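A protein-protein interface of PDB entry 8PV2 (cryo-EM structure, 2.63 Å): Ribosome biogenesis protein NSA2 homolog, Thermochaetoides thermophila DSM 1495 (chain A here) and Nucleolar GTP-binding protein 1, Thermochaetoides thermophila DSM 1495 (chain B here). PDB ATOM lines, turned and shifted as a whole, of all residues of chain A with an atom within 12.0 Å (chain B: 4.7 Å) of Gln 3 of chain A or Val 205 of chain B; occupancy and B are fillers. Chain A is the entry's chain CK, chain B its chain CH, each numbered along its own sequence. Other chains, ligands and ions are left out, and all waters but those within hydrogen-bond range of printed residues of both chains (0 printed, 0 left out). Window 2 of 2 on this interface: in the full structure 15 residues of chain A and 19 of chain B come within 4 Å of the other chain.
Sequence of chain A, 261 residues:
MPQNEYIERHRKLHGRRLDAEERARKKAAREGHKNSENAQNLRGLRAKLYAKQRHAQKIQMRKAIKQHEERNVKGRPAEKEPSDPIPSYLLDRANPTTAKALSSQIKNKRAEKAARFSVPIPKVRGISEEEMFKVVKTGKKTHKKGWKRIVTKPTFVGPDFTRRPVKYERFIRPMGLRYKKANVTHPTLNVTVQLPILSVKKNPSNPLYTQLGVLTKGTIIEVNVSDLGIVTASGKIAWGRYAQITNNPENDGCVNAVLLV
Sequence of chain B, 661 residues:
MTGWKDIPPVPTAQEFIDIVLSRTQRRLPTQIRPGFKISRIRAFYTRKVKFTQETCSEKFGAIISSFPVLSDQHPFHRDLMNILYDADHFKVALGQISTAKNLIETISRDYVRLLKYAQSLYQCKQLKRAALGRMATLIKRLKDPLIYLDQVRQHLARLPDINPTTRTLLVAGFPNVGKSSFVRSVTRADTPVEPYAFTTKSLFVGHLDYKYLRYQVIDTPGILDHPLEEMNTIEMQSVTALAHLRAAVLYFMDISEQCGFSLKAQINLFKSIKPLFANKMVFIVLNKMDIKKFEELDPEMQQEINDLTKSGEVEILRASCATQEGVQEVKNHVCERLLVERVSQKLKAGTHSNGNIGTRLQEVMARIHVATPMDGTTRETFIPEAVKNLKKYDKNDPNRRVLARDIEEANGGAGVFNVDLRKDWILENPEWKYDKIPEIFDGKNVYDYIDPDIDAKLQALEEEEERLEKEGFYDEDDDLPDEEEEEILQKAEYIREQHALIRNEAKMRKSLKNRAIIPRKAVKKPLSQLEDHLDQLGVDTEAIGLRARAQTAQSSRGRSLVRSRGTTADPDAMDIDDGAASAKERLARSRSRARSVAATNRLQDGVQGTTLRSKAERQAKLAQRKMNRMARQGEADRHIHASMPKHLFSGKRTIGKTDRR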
ATOM      1  N   PRO A   2       0.735  -5.454  26.608  1.00  0.00           N
ATOM      2  CA  PRO A   2       1.432  -4.745  27.673  1.00  0.00           C
ATOM      3  C   PRO A   2       2.638  -4.013  27.114  1.00  0.00           C
ATOM      4  O   PRO A   2       3.084  -4.335  26.017  1.00  0.00           O
ATOM      5  CB  PRO A   2       1.827  -5.869  28.620  1.00  0.00           C
ATOM      6  CG  PRO A   2       2.077  -7.001  27.731  1.00  0.00           C
ATOM      7  CD  PRO A   2       1.120  -6.871  26.573  1.00  0.00           C
ATOM      8  N   GLN A   3       3.134  -3.019  27.836  1.00  0.00           N
ATOM      9  CA  GLN A   3       4.206  -2.177  27.334  1.00  0.00           C
ATOM     10  C   GLN A   3       5.153  -1.824  28.468  1.00  0.00           C
ATOM     11  O   GLN A   3       4.743  -1.715  29.627  1.00  0.00           O
ATOM     12  CB  GLN A   3       3.647  -0.905  26.691  1.00  0.00           C
ATOM     13  CG  GLN A   3       2.502  -0.288  27.471  1.00  0.00           C
ATOM     14  CD  GLN A   3       1.722   0.718  26.664  1.00  0.00           C
ATOM     15  OE1 GLN A   3       2.224   1.272  25.692  1.00  0.00           O
ATOM     16  NE2 GLN A   3       0.484   0.959  27.059  1.00  0.00           N
ATOM     17  N   ASN A   4       6.419  -1.642  28.108  1.00  0.00           N
ATOM     18  CA  ASN A   4       7.509  -1.185  28.988  1.00  0.00           C
ATOM     19  C   ASN A   4       7.688  -2.223  30.101  1.00  0.00           C
ATOM     20  O   ASN A   4       7.668  -3.429  29.824  1.00  0.00           O
ATOM     21  CB  ASN A   4       7.230   0.228  29.442  1.00  0.00           C
ATOM     22  CG  ASN A   4       7.057   1.178  28.279  1.00  0.00           C
ATOM     23  OD1 ASN A   4       7.869   1.193  27.358  1.00  0.00           O
ATOM     24  ND2 ASN A   4       5.997   1.972  28.310  1.00  0.00           N
ATOM     25  N   GLU A   5       7.861  -1.810  31.353  1.00  0.00           N
ATOM     26  CA  GLU A   5       8.171  -2.747  32.433  1.00  0.00           C
ATOM     27  C   GLU A   5       6.886  -3.251  33.091  1.00  0.00           C
ATOM     28  O   GLU A   5       6.558  -2.937  34.239  1.00  0.00           O
ATOM     29  CB  GLU A   5       9.096  -2.095  33.449  1.00  0.00           C
ATOM     30  CG  GLU A   5      10.551  -2.112  33.051  1.00  0.00           C
ATOM     31  CD  GLU A   5      10.894  -1.012  32.076  1.00  0.00           C
ATOM     32  OE1 GLU A   5      10.077  -0.082  31.923  1.00  0.00           O
ATOM     33  OE2 GLU A   5      11.976  -1.072  31.459  1.00  0.00           O
ATOM     34  N   TYR A   6       6.166  -4.086  32.340  1.00  0.00           N
ATOM     35  CA  TYR A   6       4.835  -4.487  32.782  1.00  0.00           C
ATOM     36  C   TYR A   6       4.884  -5.552  33.875  1.00  0.00           C
ATOM     37  O   TYR A   6       4.022  -5.566  34.758  1.00  0.00           O
ATOM     38  CB  TYR A   6       3.990  -4.944  31.591  1.00  0.00           C
ATOM     39  CG  TYR A   6       4.621  -5.934  30.646  1.00  0.00           C
ATOM     40  CD1 TYR A   6       4.498  -7.301  30.851  1.00  0.00           C
ATOM     41  CD2 TYR A   6       5.290  -5.503  29.513  1.00  0.00           C
ATOM     42  CE1 TYR A   6       5.049  -8.204  29.970  1.00  0.00           C
ATOM     43  CE2 TYR A   6       5.846  -6.397  28.632  1.00  0.00           C
ATOM     44  CZ  TYR A   6       5.721  -7.744  28.863  1.00  0.00           C
ATOM     45  OH  TYR A   6       6.281  -8.632  27.979  1.00  0.00           O
ATOM     46  N   ILE A   7       5.880  -6.440  33.856  1.00  0.00           N
ATOM     47  CA  ILE A   7       5.992  -7.425  34.933  1.00  0.00           C
ATOM     48  C   ILE A   7       6.425  -6.752  36.231  1.00  0.00           C
ATOM     49  O   ILE A   7       5.935  -7.094  37.315  1.00  0.00           O
ATOM     50  CB  ILE A   7       6.934  -8.575  34.521  1.00  0.00           C
ATOM     51  CG1 ILE A   7       6.221  -9.525  33.552  1.00  0.00           C
ATOM     52  CG2 ILE A   7       7.454  -9.350  35.718  1.00  0.00           C
ATOM     53  CD1 ILE A   7       5.036 -10.237  34.149  1.00  0.00           C
ATOM     54  N   GLU A   8       7.326  -5.770  36.144  1.00  0.00           N
ATOM     55  CA  GLU A   8       7.686  -4.992  37.327  1.00  0.00           C
ATOM     56  C   GLU A   8       6.495  -4.212  37.866  1.00  0.00           C
ATOM     57  O   GLU A   8       6.305  -4.127  39.085  1.00  0.00           O
ATOM     58  CB  GLU A   8       8.839  -4.044  37.007  1.00  0.00           C
ATOM     59  CG  GLU A   8      10.157  -4.741  36.755  1.00  0.00           C
ATOM     60  CD  GLU A   8      11.228  -3.792  36.272  1.00  0.00           C
ATOM     61  OE1 GLU A   8      11.070  -2.569  36.469  1.00  0.00           O
ATOM     62  OE2 GLU A   8      12.225  -4.265  35.689  1.00  0.00           O
ATOM     63  N   ARG A   9       5.682  -3.636  36.979  1.00  0.00           N
ATOM     64  CA  ARG A   9       4.485  -2.935  37.434  1.00  0.00           C
ATOM     65  C   ARG A   9       3.486  -3.900  38.059  1.00  0.00           C
ATOM     66  O   ARG A   9       2.818  -3.560  39.042  1.00  0.00           O
ATOM     67  CB  ARG A   9       3.856  -2.164  36.274  1.00  0.00           C
ATOM     68  CG  ARG A   9       2.547  -1.493  36.623  1.00  0.00           C
ATOM     69  CD  ARG A   9       2.443  -0.115  36.023  1.00  0.00           C
ATOM     70  NE  ARG A   9       1.198   0.540  36.402  1.00  0.00           N
ATOM     71  CZ  ARG A   9       1.014   1.196  37.539  1.00  0.00           C
ATOM     72  NH1 ARG A   9       1.982   1.318  38.431  1.00  0.00           N
ATOM     73  NH2 ARG A   9      -0.173   1.741  37.788  1.00  0.00           N
ATOM     74  N   HIS A  10       3.385  -5.114  37.515  1.00  0.00           N
ATOM     75  CA  HIS A  10       2.510  -6.125  38.096  1.00  0.00           C
ATOM     76  C   HIS A  10       2.984  -6.533  39.481  1.00  0.00           C
ATOM     77  O   HIS A  10       2.170  -6.759  40.381  1.00  0.00           O
ATOM     78  CB  HIS A  10       2.438  -7.344  37.179  1.00  0.00           C
ATOM     79  CG  HIS A  10       1.511  -8.408  37.670  1.00  0.00           C
ATOM     80  ND1 HIS A  10       0.156  -8.383  37.427  1.00  0.00           N
ATOM     81  CD2 HIS A  10       1.741  -9.523  38.400  1.00  0.00           C
ATOM     82  CE1 HIS A  10      -0.408  -9.438  37.985  1.00  0.00           C
ATOM     83  NE2 HIS A  10       0.532 -10.146  38.582  1.00  0.00           N
ATOM     84  N   ARG A  11       4.299  -6.644  39.664  1.00  0.00           N
ATOM     85  CA  ARG A  11       4.859  -6.930  40.980  1.00  0.00           C
ATOM     86  C   ARG A  11       4.585  -5.794  41.956  1.00  0.00           C
ATOM     87  O   ARG A  11       4.295  -6.033  43.132  1.00  0.00           O
ATOM     88  CB  ARG A  11       6.361  -7.182  40.858  1.00  0.00           C
ATOM     89  CG  ARG A  11       7.070  -7.469  42.164  1.00  0.00           C
ATOM     90  CD  ARG A  11       8.482  -7.957  41.920  1.00  0.00           C
ATOM     91  NE  ARG A  11       9.289  -7.868  43.130  1.00  0.00           N
ATOM     92  CZ  ARG A  11      10.181  -8.773  43.509  1.00  0.00           C
ATOM     93  NH1 ARG A  11      10.450  -9.831  42.763  1.00  0.00           N
ATOM     94  NH2 ARG A  11      10.827  -8.604  44.658  1.00  0.00           N
ATOM     95  N   LYS A  12       4.667  -4.549  41.486  1.00  0.00           N
ATOM     96  CA  LYS A  12       4.406  -3.409  42.362  1.00  0.00           C
ATOM     97  C   LYS A  12       2.932  -3.319  42.747  1.00  0.00           C
ATOM     98  O   LYS A  12       2.605  -2.922  43.870  1.00  0.00           O
ATOM     99  CB  LYS A  12       4.863  -2.117  41.694  1.00  0.00           C
ATOM    100  CG  LYS A  12       6.364  -2.004  41.533  1.00  0.00           C
ATOM    101  CD  LYS A  12       6.751  -0.706  40.844  1.00  0.00           C
ATOM    102  CE  LYS A  12       8.236  -0.672  40.507  1.00  0.00           C
ATOM    103  NZ  LYS A  12       9.099  -0.612  41.716  1.00  0.00           N
ATOM    104  N   LEU A  13       2.030  -3.679  41.836  1.00  0.00           N
ATOM    105  CA  LEU A  13       0.607  -3.519  42.121  1.00  0.00           C
ATOM    106  C   LEU A  13       0.003  -4.719  42.841  1.00  0.00           C
ATOM    107  O   LEU A  13      -0.899  -4.542  43.664  1.00  0.00           O
ATOM    108  CB  LEU A  13      -0.163  -3.255  40.830  1.00  0.00           C
ATOM    109  CG  LEU A  13       0.113  -1.903  40.184  1.00  0.00           C
ATOM    110  CD1 LEU A  13      -0.585  -1.807  38.845  1.00  0.00           C
ATOM    111  CD2 LEU A  13      -0.333  -0.792  41.109  1.00  0.00           C
ATOM    112  N   ARG B 158       9.536  -5.464  24.552  1.00  0.00           N
ATOM    113  CA  ARG B 158       8.587  -4.759  25.405  1.00  0.00           C
ATOM    114  C   ARG B 158       8.210  -3.368  24.893  1.00  0.00           C
ATOM    115  O   ARG B 158       7.486  -2.651  25.587  1.00  0.00           O
ATOM    116  CB  ARG B 158       9.132  -4.666  26.827  1.00  0.00           C
ATOM    117  CG  ARG B 158       9.457  -6.005  27.436  1.00  0.00           C
ATOM    118  CD  ARG B 158       9.609  -5.895  28.931  1.00  0.00           C
ATOM    119  NE  ARG B 158      10.492  -4.797  29.296  1.00  0.00           N
ATOM    120  CZ  ARG B 158      11.807  -4.897  29.420  1.00  0.00           C
ATOM    121  NH1 ARG B 158      12.436  -6.039  29.205  1.00  0.00           N
ATOM    122  NH2 ARG B 158      12.509  -3.823  29.761  1.00  0.00           N
ATOM    123  N   PRO B 160       6.133  -0.488  22.926  1.00  0.00           N
ATOM    124  CA  PRO B 160       4.754  -0.364  22.440  1.00  0.00           C
ATOM    125  C   PRO B 160       4.700  -0.347  20.920  1.00  0.00           C
ATOM    126  O   PRO B 160       5.672  -0.002  20.247  1.00  0.00           O
ATOM    127  CB  PRO B 160       4.294   0.974  23.026  1.00  0.00           C
ATOM    128  CG  PRO B 160       5.534   1.736  23.229  1.00  0.00           C
ATOM    129  CD  PRO B 160       6.578   0.736  23.611  1.00  0.00           C
ATOM    130  N   ASP B 161       3.543  -0.713  20.379  1.00  0.00           N
ATOM    131  CA  ASP B 161       3.340  -0.756  18.934  1.00  0.00           C
ATOM    132  C   ASP B 161       2.648   0.534  18.517  1.00  0.00           C
ATOM    133  O   ASP B 161       1.486   0.767  18.854  1.00  0.00           O
ATOM    134  CB  ASP B 161       2.522  -1.978  18.546  1.00  0.00           C
ATOM    135  CG  ASP B 161       2.592  -2.280  17.069  1.00  0.00           C
ATOM    136  OD1 ASP B 161       3.398  -1.634  16.367  1.00  0.00           O
ATOM    137  OD2 ASP B 161       1.833  -3.155  16.603  1.00  0.00           O
ATOM    138  N   ILE B 162       3.358   1.374  17.777  1.00  0.00           N
ATOM    139  CA  ILE B 162       2.860   2.683  17.379  1.00  0.00           C
ATOM    140  C   ILE B 162       2.812   2.725  15.861  1.00  0.00           C
ATOM    141  O   ILE B 162       3.840   2.581  15.191  1.00  0.00           O
ATOM    142  CB  ILE B 162       3.723   3.815  17.946  1.00  0.00           C
ATOM    143  CG1 ILE B 162       3.627   3.828  19.471  1.00  0.00           C
ATOM    144  CG2 ILE B 162       3.294   5.143  17.372  1.00  0.00           C
ATOM    145  CD1 ILE B 162       4.503   4.844  20.134  1.00  0.00           C
ATOM    146  N   ALA B 189      -4.991   2.480  28.780  1.00  0.00           N
ATOM    147  CA  ALA B 189      -3.572   2.243  29.012  1.00  0.00           C
ATOM    148  C   ALA B 189      -3.223   2.378  30.489  1.00  0.00           C
ATOM    149  O   ALA B 189      -3.793   3.206  31.204  1.00  0.00           O
ATOM    150  CB  ALA B 189      -2.737   3.218  28.186  1.00  0.00           C
ATOM    151  N   LEU B 203       7.554   6.040  26.018  1.00  0.00           N
ATOM    152  CA  LEU B 203       6.316   6.302  25.304  1.00  0.00           C
ATOM    153  C   LEU B 203       5.276   5.255  25.676  1.00  0.00           C
ATOM    154  O   LEU B 203       5.522   4.054  25.550  1.00  0.00           O
ATOM    155  CB  LEU B 203       6.559   6.298  23.798  1.00  0.00           C
ATOM    156  CG  LEU B 203       7.505   7.355  23.233  1.00  0.00           C
ATOM    157  CD1 LEU B 203       7.708   7.134  21.752  1.00  0.00           C
ATOM    158  CD2 LEU B 203       6.972   8.743  23.492  1.00  0.00           C
ATOM    159  N   PHE B 204       4.121   5.706  26.150  1.00  0.00           N
ATOM    160  CA  PHE B 204       2.974   4.839  26.370  1.00  0.00           C
ATOM    161  C   PHE B 204       1.935   5.145  25.304  1.00  0.00           C
ATOM    162  O   PHE B 204       1.869   6.263  24.796  1.00  0.00           O
ATOM    163  CB  PHE B 204       2.358   5.040  27.760  1.00  0.00           C
ATOM    164  CG  PHE B 204       3.092   4.343  28.866  1.00  0.00           C
ATOM    165  CD1 PHE B 204       4.221   4.909  29.435  1.00  0.00           C
ATOM    166  CD2 PHE B 204       2.643   3.130  29.350  1.00  0.00           C
ATOM    167  CE1 PHE B 204       4.893   4.272  30.456  1.00  0.00           C
ATOM    168  CE2 PHE B 204       3.311   2.489  30.376  1.00  0.00           C
ATOM    169  CZ  PHE B 204       4.434   3.063  30.930  1.00  0.00           C
ATOM    170  N   VAL B 205       1.123   4.155  24.958  1.00  0.00           N
ATOM    171  CA  VAL B 205       0.089   4.335  23.948  1.00  0.00           C
ATOM    172  C   VAL B 205      -1.199   3.675  24.422  1.00  0.00           C
ATOM    173  O   VAL B 205      -1.181   2.591  25.012  1.00  0.00           O
ATOM    174  CB  VAL B 205       0.552   3.799  22.572  1.00  0.00           C
ATOM    175  CG1 VAL B 205       0.931   2.349  22.644  1.00  0.00           C
ATOM    176  CG2 VAL B 205      -0.503   4.021  21.505  1.00  0.00           C
ATOM    177  N   GLY B 206      -2.316   4.378  24.223  1.00  0.00           N
ATOM    178  CA  GLY B 206      -3.627   3.815  24.436  1.00  0.00           C
ATOM    179  C   GLY B 206      -4.478   4.008  23.195  1.00  0.00           C
ATOM    180  O   GLY B 206      -4.037   4.585  22.205  1.00  0.00           O
ATOM    181  N   HIS B 207      -5.712   3.522  23.267  1.00  0.00           N
ATOM    182  CA  HIS B 207      -6.608   3.581  22.125  1.00  0.00           C
ATOM    183  C   HIS B 207      -7.995   4.010  22.573  1.00  0.00           C
ATOM    184  O   HIS B 207      -8.398   3.788  23.716  1.00  0.00           O
ATOM    185  CB  HIS B 207      -6.678   2.235  21.403  1.00  0.00           C
ATOM    186  CG  HIS B 207      -5.391   1.826  20.760  1.00  0.00           C
ATOM    187  ND1 HIS B 207      -4.341   1.286  21.470  1.00  0.00           N
ATOM    188  CD2 HIS B 207      -4.990   1.863  19.469  1.00  0.00           C
ATOM    189  CE1 HIS B 207      -3.345   1.020  20.646  1.00  0.00           C
ATOM    190  NE2 HIS B 207      -3.713   1.361  19.425  1.00  0.00           N
ATOM    191  N   GLN B 216      -5.317   6.399  18.270  1.00  0.00           N
ATOM    192  CA  GLN B 216      -4.268   6.045  19.213  1.00  0.00           C
ATOM    193  C   GLN B 216      -3.740   7.303  19.895  1.00  0.00           C
ATOM    194  O   GLN B 216      -3.558   8.340  19.252  1.00  0.00           O
ATOM    195  CB  GLN B 216      -3.147   5.258  18.527  1.00  0.00           C
ATOM    196  CG  GLN B 216      -2.347   6.000  17.495  1.00  0.00           C
ATOM    197  CD  GLN B 216      -1.182   5.195  16.972  1.00  0.00           C
ATOM    198  OE1 GLN B 216      -1.014   4.028  17.318  1.00  0.00           O
ATOM    199  NE2 GLN B 216      -0.367   5.814  16.131  1.00  0.00           N
ATOM    200  N   VAL B 217      -3.538   7.212  21.206  1.00  0.00           N
ATOM    201  CA  VAL B 217      -3.154   8.334  22.052  1.00  0.00           C
ATOM    202  C   VAL B 217      -1.787   8.031  22.644  1.00  0.00           C
ATOM    203  O   VAL B 217      -1.606   6.998  23.290  1.00  0.00           O
ATOM    204  CB  VAL B 217      -4.188   8.573  23.166  1.00  0.00           C
ATOM    205  CG1 VAL B 217      -3.799   9.760  24.017  1.00  0.00           C
ATOM    206  CG2 VAL B 217      -5.556   8.764  22.570  1.00  0.00           C
ATOM    207  N   ILE B 218      -0.835   8.931  22.433  1.00  0.00           N
ATOM    208  CA  ILE B 218       0.553   8.703  22.814  1.00  0.00           C
ATOM    209  C   ILE B 218       0.917   9.627  23.966  1.00  0.00           C
ATOM    210  O   ILE B 218       0.971  10.854  23.805  1.00  0.00           O
ATOM    211  CB  ILE B 218       1.500   8.892  21.621  1.00  0.00           C
ATOM    212  CG1 ILE B 218       1.147   7.885  20.530  1.00  0.00           C
ATOM    213  CG2 ILE B 218       2.943   8.732  22.053  1.00  0.00           C
ATOM    214  CD1 ILE B 218       1.907   8.068  19.265  1.00  0.00           C
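The backbone NH (N) of Asn 4 of chain A sits at hydrogen-bond distance from the backbone carbonyl oxygen (O) of Arg 158 of chain B. The guanidinium group of Arg 158 of chain B is in salt-bridge range of the side-chain carboxylate of Glu 5 of chain A (3.3 Å). The side-chain amide nitrogen of Asn 4 of chain A lies within hydrogen-bond range of the backbone carbonyl oxygen of Leu 203 of chain B. NE2 of Gln 3 of chain A is in hydrogen-bond range of O of Val 205 of chain B (3.1 Å).
Among the printed residues, merely in contact across the chains: Gln 3 of chain A with Arg 158 of chain B, Gln 3 of chain A with Pro 160 of chain B, Gln 3 of chain A with Phe 204 of chain B, Asn 4 of chain A with Pro 160 of chain B, Asn 4 of chain A with Phe 204 of chain B and Tyr 6 of chain A with Arg 158 of chain B.
Gln 3 of chain A touches just these residues of chain B: Arg 158, Pro 160, Phe 204 and Val 205. Printed residues of chain B within 4 Å of Tyr 6 of chain A: Arg 158 (3.8 Å). Ile 7 of chain A touches none of the printed residues of chain B. Printed residues of chain A within 4 Å of Arg 158 of chain B: Gln 3, Asn 4, Glu 5 and Tyr 6. No residue of chain A comes within 4 Å of Ala 189 of chain B. Of chain A, only Gln 3 (3.7 Å) and Asn 4 (3.2 Å) come within 4 Å of Phe 204 of chain B. No residue of chain A comes within 4 Å of Gly 206 of chain B. His 207 of chain B touches none of the printed residues of chain A. No residue of chain A comes within 4 Å of Gln 216 of chain B. Val 217 of chain B touches none of the printed residues of chain A. The nearest residue of chain A that does not touch Val 205 of chain B is Asn 4 of chain A (6.3 Å).
Hydrophobic or aromatic side chains of chain B that line the printed part of chain A: Pro 160, Phe 204 and Val 205.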
